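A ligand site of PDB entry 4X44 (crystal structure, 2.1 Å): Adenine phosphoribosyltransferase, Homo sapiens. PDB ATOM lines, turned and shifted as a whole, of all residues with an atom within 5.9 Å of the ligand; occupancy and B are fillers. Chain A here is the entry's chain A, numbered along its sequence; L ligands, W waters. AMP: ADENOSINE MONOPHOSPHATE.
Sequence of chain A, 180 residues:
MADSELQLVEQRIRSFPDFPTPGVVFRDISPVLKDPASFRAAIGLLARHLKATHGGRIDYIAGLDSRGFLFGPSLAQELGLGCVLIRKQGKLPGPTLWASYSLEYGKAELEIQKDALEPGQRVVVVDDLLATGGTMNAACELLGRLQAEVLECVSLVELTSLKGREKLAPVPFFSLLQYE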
ATOM      1  N   PHE A  19      -3.982   2.462 -38.454  1.00  0.00           N
ATOM      2  CA  PHE A  19      -3.344   2.413 -37.140  1.00  0.00           C
ATOM      3  C   PHE A  19      -3.975   1.293 -36.313  1.00  0.00           C
ATOM      4  O   PHE A  19      -5.194   1.164 -36.276  1.00  0.00           O
ATOM      5  CB  PHE A  19      -3.475   3.750 -36.409  1.00  0.00           C
ATOM      6  CG  PHE A  19      -2.746   3.788 -35.095  1.00  0.00           C
ATOM      7  CD1 PHE A  19      -1.401   4.098 -35.041  1.00  0.00           C
ATOM      8  CD2 PHE A  19      -3.417   3.502 -33.918  1.00  0.00           C
ATOM      9  CE1 PHE A  19      -0.730   4.127 -33.826  1.00  0.00           C
ATOM     10  CE2 PHE A  19      -2.749   3.524 -32.699  1.00  0.00           C
ATOM     11  CZ  PHE A  19      -1.409   3.839 -32.661  1.00  0.00           C
ATOM     12  N   VAL A  24      -6.356  -1.122 -40.876  1.00  0.00           N
ATOM     13  CA  VAL A  24      -7.129  -1.048 -39.644  1.00  0.00           C
ATOM     14  C   VAL A  24      -7.519   0.390 -39.317  1.00  0.00           C
ATOM     15  O   VAL A  24      -6.670   1.279 -39.273  1.00  0.00           O
ATOM     16  CB  VAL A  24      -6.341  -1.640 -38.457  1.00  0.00           C
ATOM     17  CG1 VAL A  24      -7.156  -1.534 -37.169  1.00  0.00           C
ATOM     18  CG2 VAL A  24      -5.966  -3.084 -38.736  1.00  0.00           C
ATOM     19  N   VAL A  25      -8.811   0.603 -39.082  1.00  0.00           N
ATOM     20  CA  VAL A  25      -9.305   1.922 -38.692  1.00  0.00           C
ATOM     21  C   VAL A  25      -9.416   2.013 -37.173  1.00  0.00           C
ATOM     22  O   VAL A  25     -10.264   1.362 -36.561  1.00  0.00           O
ATOM     23  CB  VAL A  25     -10.680   2.207 -39.318  1.00  0.00           C
ATOM     24  CG1 VAL A  25     -11.191   3.571 -38.875  1.00  0.00           C
ATOM     25  CG2 VAL A  25     -10.588   2.133 -40.837  1.00  0.00           C
ATOM     26  N   PHE A  26      -8.558   2.826 -36.570  1.00  0.00           N
ATOM     27  CA  PHE A  26      -8.547   3.005 -35.118  1.00  0.00           C
ATOM     28  C   PHE A  26      -9.641   3.975 -34.683  1.00  0.00           C
ATOM     29  O   PHE A  26      -9.724   5.097 -35.185  1.00  0.00           O
ATOM     30  CB  PHE A  26      -7.172   3.507 -34.657  1.00  0.00           C
ATOM     31  CG  PHE A  26      -6.996   3.508 -33.168  1.00  0.00           C
ATOM     32  CD1 PHE A  26      -7.371   4.612 -32.411  1.00  0.00           C
ATOM     33  CD2 PHE A  26      -6.440   2.416 -32.524  1.00  0.00           C
ATOM     34  CE1 PHE A  26      -7.204   4.613 -31.041  1.00  0.00           C
ATOM     35  CE2 PHE A  26      -6.264   2.415 -31.150  1.00  0.00           C
ATOM     36  CZ  PHE A  26      -6.647   3.516 -30.405  1.00  0.00           C
ATOM     37  N   ARG A  27     -10.475   3.536 -33.747  1.00  0.00           N
ATOM     38  CA  ARG A  27     -11.519   4.361 -33.173  1.00  0.00           C
ATOM     39  C   ARG A  27     -11.039   4.928 -31.845  1.00  0.00           C
ATOM     40  O   ARG A  27     -10.830   4.180 -30.885  1.00  0.00           O
ATOM     41  CB  ARG A  27     -12.797   3.545 -32.956  1.00  0.00           C
ATOM     42  CG  ARG A  27     -13.208   2.702 -34.157  1.00  0.00           C
ATOM     43  CD  ARG A  27     -13.550   3.578 -35.342  1.00  0.00           C
ATOM     44  NE  ARG A  27     -14.022   2.789 -36.480  1.00  0.00           N
ATOM     45  CZ  ARG A  27     -14.566   3.315 -37.566  1.00  0.00           C
ATOM     46  NH1 ARG A  27     -14.710   4.629 -37.675  1.00  0.00           N
ATOM     47  NH2 ARG A  27     -14.974   2.525 -38.552  1.00  0.00           N
ATOM     48  N   ASP A  28     -10.869   6.245 -31.789  1.00  0.00           N
ATOM     49  CA  ASP A  28     -10.311   6.899 -30.604  1.00  0.00           C
ATOM     50  C   ASP A  28     -11.395   7.518 -29.729  1.00  0.00           C
ATOM     51  O   ASP A  28     -12.144   8.387 -30.183  1.00  0.00           O
ATOM     52  CB  ASP A  28      -9.296   7.952 -31.037  1.00  0.00           C
ATOM     53  CG  ASP A  28      -8.550   8.568 -29.870  1.00  0.00           C
ATOM     54  OD1 ASP A  28      -8.591   7.996 -28.761  1.00  0.00           O
ATOM     55  OD2 ASP A  28      -7.899   9.612 -30.065  1.00  0.00           O
ATOM     56  N   ASP A  65      -7.422  -3.247 -18.470  1.00  0.00           N
ATOM     57  CA  ASP A  65      -6.182  -2.566 -18.836  1.00  0.00           C
ATOM     58  C   ASP A  65      -6.156  -2.394 -20.357  1.00  0.00           C
ATOM     59  O   ASP A  65      -6.304  -3.374 -21.086  1.00  0.00           O
ATOM     60  CB  ASP A  65      -5.003  -3.449 -18.420  1.00  0.00           C
ATOM     61  CG  ASP A  65      -3.796  -2.658 -17.945  1.00  0.00           C
ATOM     62  OD1 ASP A  65      -3.680  -1.468 -18.279  1.00  0.00           O
ATOM     63  OD2 ASP A  65      -2.957  -3.249 -17.241  1.00  0.00           O
ATOM     64  N   SER A  66      -5.978  -1.169 -20.853  1.00  0.00           N
ATOM     65  CA  SER A  66      -5.788   0.028 -20.045  1.00  0.00           C
ATOM     66  C   SER A  66      -6.929   1.034 -20.246  1.00  0.00           C
ATOM     67  O   SER A  66      -7.272   1.774 -19.330  1.00  0.00           O
ATOM     68  CB  SER A  66      -4.461   0.705 -20.384  1.00  0.00           C
ATOM     69  OG  SER A  66      -4.449   1.161 -21.733  1.00  0.00           O
ATOM     70  N   ARG A  67      -7.501   1.054 -21.438  1.00  0.00           N
ATOM     71  CA  ARG A  67      -8.522   2.038 -21.782  1.00  0.00           C
ATOM     72  C   ARG A  67      -9.841   1.785 -21.058  1.00  0.00           C
ATOM     73  O   ARG A  67     -10.671   2.693 -20.928  1.00  0.00           O
ATOM     74  CB  ARG A  67      -8.730   2.107 -23.294  1.00  0.00           C
ATOM     75  CG  ARG A  67      -7.663   2.927 -24.003  1.00  0.00           C
ATOM     76  CD  ARG A  67      -7.833   2.879 -25.510  1.00  0.00           C
ATOM     77  NE  ARG A  67      -7.124   1.751 -26.116  1.00  0.00           N
ATOM     78  CZ  ARG A  67      -7.523   1.126 -27.209  1.00  0.00           C
ATOM     79  NH1 ARG A  67      -8.628   1.512 -27.826  1.00  0.00           N
ATOM     80  NH2 ARG A  67      -6.816   0.110 -27.693  1.00  0.00           N
ATOM     81  N   LYS A  88      -2.961  -6.233 -17.891  1.00  0.00           N
ATOM     82  CA  LYS A  88      -2.010  -6.916 -18.750  1.00  0.00           C
ATOM     83  C   LYS A  88      -1.061  -7.691 -17.851  1.00  0.00           C
ATOM     84  O   LYS A  88      -0.862  -7.339 -16.691  1.00  0.00           O
ATOM     85  CB  LYS A  88      -1.255  -5.917 -19.615  1.00  0.00           C
ATOM     86  CG  LYS A  88      -2.117  -5.166 -20.615  1.00  0.00           C
ATOM     87  CD  LYS A  88      -2.751  -6.117 -21.627  1.00  0.00           C
ATOM     88  CE  LYS A  88      -3.518  -5.368 -22.703  1.00  0.00           C
ATOM     89  NZ  LYS A  88      -4.672  -4.603 -22.158  1.00  0.00           N
ATOM     90  N   ALA A 108      -4.482 -12.038 -26.825  1.00  0.00           N
ATOM     91  CA  ALA A 108      -5.245 -11.553 -25.679  1.00  0.00           C
ATOM     92  C   ALA A 108      -4.624 -12.129 -24.412  1.00  0.00           C
ATOM     93  O   ALA A 108      -4.852 -13.286 -24.069  1.00  0.00           O
ATOM     94  CB  ALA A 108      -6.696 -11.957 -25.801  1.00  0.00           C
ATOM     95  N   ASP A 127     -14.876  -2.311 -21.202  1.00  0.00           N
ATOM     96  CA  ASP A 127     -13.728  -1.850 -21.958  1.00  0.00           C
ATOM     97  C   ASP A 127     -14.204  -0.724 -22.867  1.00  0.00           C
ATOM     98  O   ASP A 127     -15.400  -0.457 -22.939  1.00  0.00           O
ATOM     99  CB  ASP A 127     -13.131  -2.995 -22.783  1.00  0.00           C
ATOM    100  CG  ASP A 127     -11.650  -2.804 -23.070  1.00  0.00           C
ATOM    101  OD1 ASP A 127     -11.130  -1.714 -22.765  1.00  0.00           O
ATOM    102  OD2 ASP A 127     -11.017  -3.751 -23.584  1.00  0.00           O
ATOM    103  N   ASP A 128     -13.289  -0.051 -23.551  1.00  0.00           N
ATOM    104  CA  ASP A 128     -13.693   1.039 -24.438  1.00  0.00           C
ATOM    105  C   ASP A 128     -14.297   0.529 -25.737  1.00  0.00           C
ATOM    106  O   ASP A 128     -15.258   1.098 -26.249  1.00  0.00           O
ATOM    107  CB  ASP A 128     -12.531   1.996 -24.709  1.00  0.00           C
ATOM    108  CG  ASP A 128     -11.419   1.368 -25.539  1.00  0.00           C
ATOM    109  OD1 ASP A 128     -11.145   0.161 -25.365  1.00  0.00           O
ATOM    110  OD2 ASP A 128     -10.823   2.084 -26.371  1.00  0.00           O
ATOM    111  N   LEU A 129     -13.742  -0.562 -26.261  1.00  0.00           N
ATOM    112  CA  LEU A 129     -14.151  -1.061 -27.569  1.00  0.00           C
ATOM    113  C   LEU A 129     -14.135  -2.593 -27.646  1.00  0.00           C
ATOM    114  O   LEU A 129     -13.218  -3.235 -27.144  1.00  0.00           O
ATOM    115  CB  LEU A 129     -13.246  -0.479 -28.658  1.00  0.00           C
ATOM    116  CG  LEU A 129     -13.485  -0.827 -30.130  1.00  0.00           C
ATOM    117  CD1 LEU A 129     -13.135   0.353 -31.004  1.00  0.00           C
ATOM    118  CD2 LEU A 129     -12.675  -2.050 -30.560  1.00  0.00           C
ATOM    119  N   LEU A 130     -15.166  -3.153 -28.285  1.00  0.00           N
ATOM    120  CA  LEU A 130     -15.197  -4.579 -28.571  1.00  0.00           C
ATOM    121  C   LEU A 130     -14.918  -4.822 -30.043  1.00  0.00           C
ATOM    122  O   LEU A 130     -15.620  -4.306 -30.914  1.00  0.00           O
ATOM    123  CB  LEU A 130     -16.557  -5.172 -28.206  1.00  0.00           C
ATOM    124  CG  LEU A 130     -16.673  -6.676 -28.472  1.00  0.00           C
ATOM    125  CD1 LEU A 130     -15.929  -7.462 -27.413  1.00  0.00           C
ATOM    126  CD2 LEU A 130     -18.126  -7.134 -28.586  1.00  0.00           C
ATOM    127  N   ALA A 131     -13.895  -5.620 -30.333  1.00  0.00           N
ATOM    128  CA  ALA A 131     -13.572  -5.979 -31.707  1.00  0.00           C
ATOM    129  C   ALA A 131     -13.867  -7.461 -31.957  1.00  0.00           C
ATOM    130  O   ALA A 131     -15.016  -7.853 -32.129  1.00  0.00           O
ATOM    131  CB  ALA A 131     -12.129  -5.649 -32.023  1.00  0.00           C
ATOM    132  N   THR A 132     -12.813  -8.284 -31.959  1.00  0.00           N
ATOM    133  CA  THR A 132     -12.979  -9.718 -32.146  1.00  0.00           C
ATOM    134  C   THR A 132     -13.579 -10.359 -30.903  1.00  0.00           C
ATOM    135  O   THR A 132     -14.229 -11.402 -30.976  1.00  0.00           O
ATOM    136  CB  THR A 132     -11.635 -10.413 -32.455  1.00  0.00           C
ATOM    137  OG1 THR A 132     -10.788 -10.365 -31.292  1.00  0.00           O
ATOM    138  CG2 THR A 132     -10.933  -9.746 -33.627  1.00  0.00           C
ATOM    139  N   GLY A 133     -13.353  -9.730 -29.759  1.00  0.00           N
ATOM    140  CA  GLY A 133     -13.857 -10.226 -28.491  1.00  0.00           C
ATOM    141  C   GLY A 133     -12.851 -11.069 -27.730  1.00  0.00           C
ATOM    142  O   GLY A 133     -13.135 -11.556 -26.640  1.00  0.00           O
ATOM    143  N   GLY A 134     -11.667 -11.233 -28.303  1.00  0.00           N
ATOM    144  CA  GLY A 134     -10.620 -12.027 -27.692  1.00  0.00           C
ATOM    145  C   GLY A 134     -10.212 -11.536 -26.310  1.00  0.00           C
ATOM    146  O   GLY A 134      -9.952 -12.323 -25.412  1.00  0.00           O
ATOM    147  N   THR A 135     -10.176 -10.214 -26.150  1.00  0.00           N
ATOM    148  CA  THR A 135      -9.776  -9.604 -24.884  1.00  0.00           C
ATOM    149  C   THR A 135     -10.831  -9.814 -23.791  1.00  0.00           C
ATOM    150  O   THR A 135     -10.507 -10.273 -22.700  1.00  0.00           O
ATOM    151  CB  THR A 135      -9.496  -8.103 -25.056  1.00  0.00           C
ATOM    152  OG1 THR A 135      -8.484  -7.924 -26.056  1.00  0.00           O
ATOM    153  CG2 THR A 135      -9.015  -7.495 -23.741  1.00  0.00           C
ATOM    154  N   MET A 136     -12.073  -9.478 -24.098  1.00  0.00           N
ATOM    155  CA  MET A 136     -13.165  -9.641 -23.144  1.00  0.00           C
ATOM    156  C   MET A 136     -13.437 -11.100 -22.819  1.00  0.00           C
ATOM    157  O   MET A 136     -13.816 -11.432 -21.696  1.00  0.00           O
ATOM    158  CB  MET A 136     -14.434  -8.960 -23.644  1.00  0.00           C
ATOM    159  CG  MET A 136     -14.561  -7.505 -23.225  1.00  0.00           C
ATOM    160  SD  MET A 136     -16.075  -6.749 -23.856  1.00  0.00           S
ATOM    161  CE  MET A 136     -15.990  -5.157 -23.038  1.00  0.00           C
ATOM    162  N   LEU A 159     -17.338  -3.066 -33.005  1.00  0.00           N
ATOM    163  CA  LEU A 159     -17.078  -3.318 -34.417  1.00  0.00           C
ATOM    164  C   LEU A 159     -17.780  -4.611 -34.821  1.00  0.00           C
ATOM    165  O   LEU A 159     -17.217  -5.703 -34.689  1.00  0.00           O
ATOM    166  CB  LEU A 159     -15.585  -3.416 -34.685  1.00  0.00           C
ATOM    167  CG  LEU A 159     -14.738  -2.273 -34.112  1.00  0.00           C
ATOM    168  CD1 LEU A 159     -13.272  -2.472 -34.432  1.00  0.00           C
ATOM    169  CD2 LEU A 159     -15.240  -0.930 -34.625  1.00  0.00           C
ATOM    170  N   LEU A 162     -16.593  -7.895 -36.840  1.00  0.00           N
ATOM    171  CA  LEU A 162     -15.594  -8.766 -36.227  1.00  0.00           C
ATOM    172  C   LEU A 162     -16.234  -9.815 -35.315  1.00  0.00           C
ATOM    173  O   LEU A 162     -15.532 -10.659 -34.755  1.00  0.00           O
ATOM    174  CB  LEU A 162     -14.564  -7.931 -35.468  1.00  0.00           C
ATOM    175  CG  LEU A 162     -13.785  -6.951 -36.353  1.00  0.00           C
ATOM    176  CD1 LEU A 162     -12.845  -6.097 -35.526  1.00  0.00           C
ATOM    177  CD2 LEU A 162     -13.033  -7.689 -37.447  1.00  0.00           C
HETATM  178  P   AMP L   1     -10.548  -7.572 -29.277  1.00  0.00           P
HETATM  179  O1P AMP L   1      -9.708  -8.560 -28.249  1.00  0.00           O
HETATM  180  O2P AMP L   1     -12.189  -7.490 -29.093  1.00  0.00           O
HETATM  181  O3P AMP L   1     -10.229  -7.954 -30.650  1.00  0.00           O
HETATM  182  O5' AMP L   1     -10.029  -6.098 -28.962  1.00  0.00           O
HETATM  183  C5' AMP L   1     -10.115  -5.577 -27.643  1.00  0.00           C
HETATM  184  C4' AMP L   1      -9.028  -4.582 -27.353  1.00  0.00           C
HETATM  185  O4' AMP L   1      -8.442  -4.130 -28.605  1.00  0.00           O
HETATM  186  C3' AMP L   1      -9.490  -3.324 -26.629  1.00  0.00           C
HETATM  187  O3' AMP L   1      -8.424  -2.806 -25.844  1.00  0.00           O
HETATM  188  C2' AMP L   1      -9.783  -2.384 -27.796  1.00  0.00           C
HETATM  189  O2' AMP L   1      -9.796  -1.012 -27.463  1.00  0.00           O
HETATM  190  C1' AMP L   1      -8.671  -2.750 -28.779  1.00  0.00           C
HETATM  191  N9  AMP L   1      -9.029  -2.540 -30.187  1.00  0.00           N
HETATM  192  C8  AMP L   1      -9.226  -3.602 -31.215  1.00  0.00           C
HETATM  193  N7  AMP L   1      -9.562  -2.969 -32.479  1.00  0.00           N
HETATM  194  C5  AMP L   1      -9.579  -1.516 -32.263  1.00  0.00           C
HETATM  195  C6  AMP L   1      -9.853  -0.367 -33.199  1.00  0.00           C
HETATM  196  N6  AMP L   1     -10.179  -0.619 -34.590  1.00  0.00           N
HETATM  197  N1  AMP L   1      -9.799   1.003 -32.689  1.00  0.00           N
HETATM  198  C2  AMP L   1      -9.462   1.263 -31.254  1.00  0.00           C
HETATM  199  N3  AMP L   1      -9.183   0.130 -30.328  1.00  0.00           N
HETATM  200  C4  AMP L   1      -9.238  -1.253 -30.841  1.00  0.00           C
HETATM  201  O   HOH W   1      -8.545  -6.603 -32.396  1.00  0.00           O
HETATM  202  O   HOH W   2      -6.576  -5.911 -30.486  1.00  0.00           O
HETATM  203  O   HOH W   3      -5.830  -1.493 -30.081  1.00  0.00           O
HETATM  204  O   HOH W   4     -12.655  -7.795 -26.469  1.00  0.00           O
HETATM  205  O   HOH W   5      -5.532  -2.933 -27.208  1.00  0.00           O
HETATM  206  O   HOH W   6     -10.032  -4.181 -34.715  1.00  0.00           O
HETATM  207  O   HOH W   7     -12.500  -5.168 -25.365  1.00  0.00           O
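Water W4 lies within hydrogen-bond range of O2P of the ligand (2.7 Å), N of Met 136 (3.0 Å) and N of Thr 135 (3.5 Å).
Water W5 lies within hydrogen-bond range of O3' of the ligand (3.2 Å) and NH2 of Arg 67 (3.3 Å).
Water W7 lies within hydrogen-bond range of OD2 of Asp 127 (2.7 Å) and O of Leu 129 (2.7 Å).
Phe 26 touches the ligand (CA to N1, 3.4 Å).
Asp 127 touches the ligand.
CD2 of Leu 129 touches C4 of the ligand (3.5 Å).
Leu 130 touches the ligand.
Leu 159 touches the ligand.
Hydrophobic or aromatic side chains that line the ligand: Phe 26, Leu 129, Ala 131 and Leu 159.
Within 4 Å of the ligand: Val 25, Phe 26, Arg 27, Arg 67, Asp 127, Asp 128, Leu 129, Leu 130, Ala 131, Thr 132, Gly 133, Gly 134, Thr 135 and Leu 159.
N of Thr 132 lies within hydrogen-bond range of O3P of the ligand (2.9 Å).
N of Ala 131 lies within hydrogen-bond range of O2P of the ligand, 2.8 Å away.
A nitrogen (N6) of the ligand lies within hydrogen-bond range of the backbone carbonyl oxygen of Val 25 (2.8 Å).
O3P of the ligand lies within hydrogen-bond range of OG1 of Thr 132.
NH1 of Arg 67 sits at hydrogen-bond distance from O2' of the ligand (2.8 Å).
OD1 of Asp 128 lies within hydrogen-bond range of O2' of the ligand (2.8 Å).
The backbone NH (N) of Gly 134 sits at hydrogen-bond distance from an oxygen (O1P) of the ligand, at 3.3 Å.
The backbone NH (N) of Arg 27 sits at hydrogen-bond distance from a nitrogen (N1) of the ligand, 2.8 Å away.
OG1 of Thr 135 sits at hydrogen-bond distance from O1P of the ligand.
An oxygen (O1P) of the ligand is in hydrogen-bond range of the backbone NH of Thr 135 (2.7 Å).
N of Gly 133 lies within hydrogen-bond range of O2P of the ligand.
OG1 of Thr 132 lies within hydrogen-bond range of N of Gly 134.
The guanidinium group (NH1) of Arg 67 lies within salt-bridge range of the side-chain carboxylate (OD2) of Asp 128 (2.7 Å).
The backbone NH of Leu 159 lies within hydrogen-bond range of the backbone carbonyl oxygen of Leu 130 (3.0 Å).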
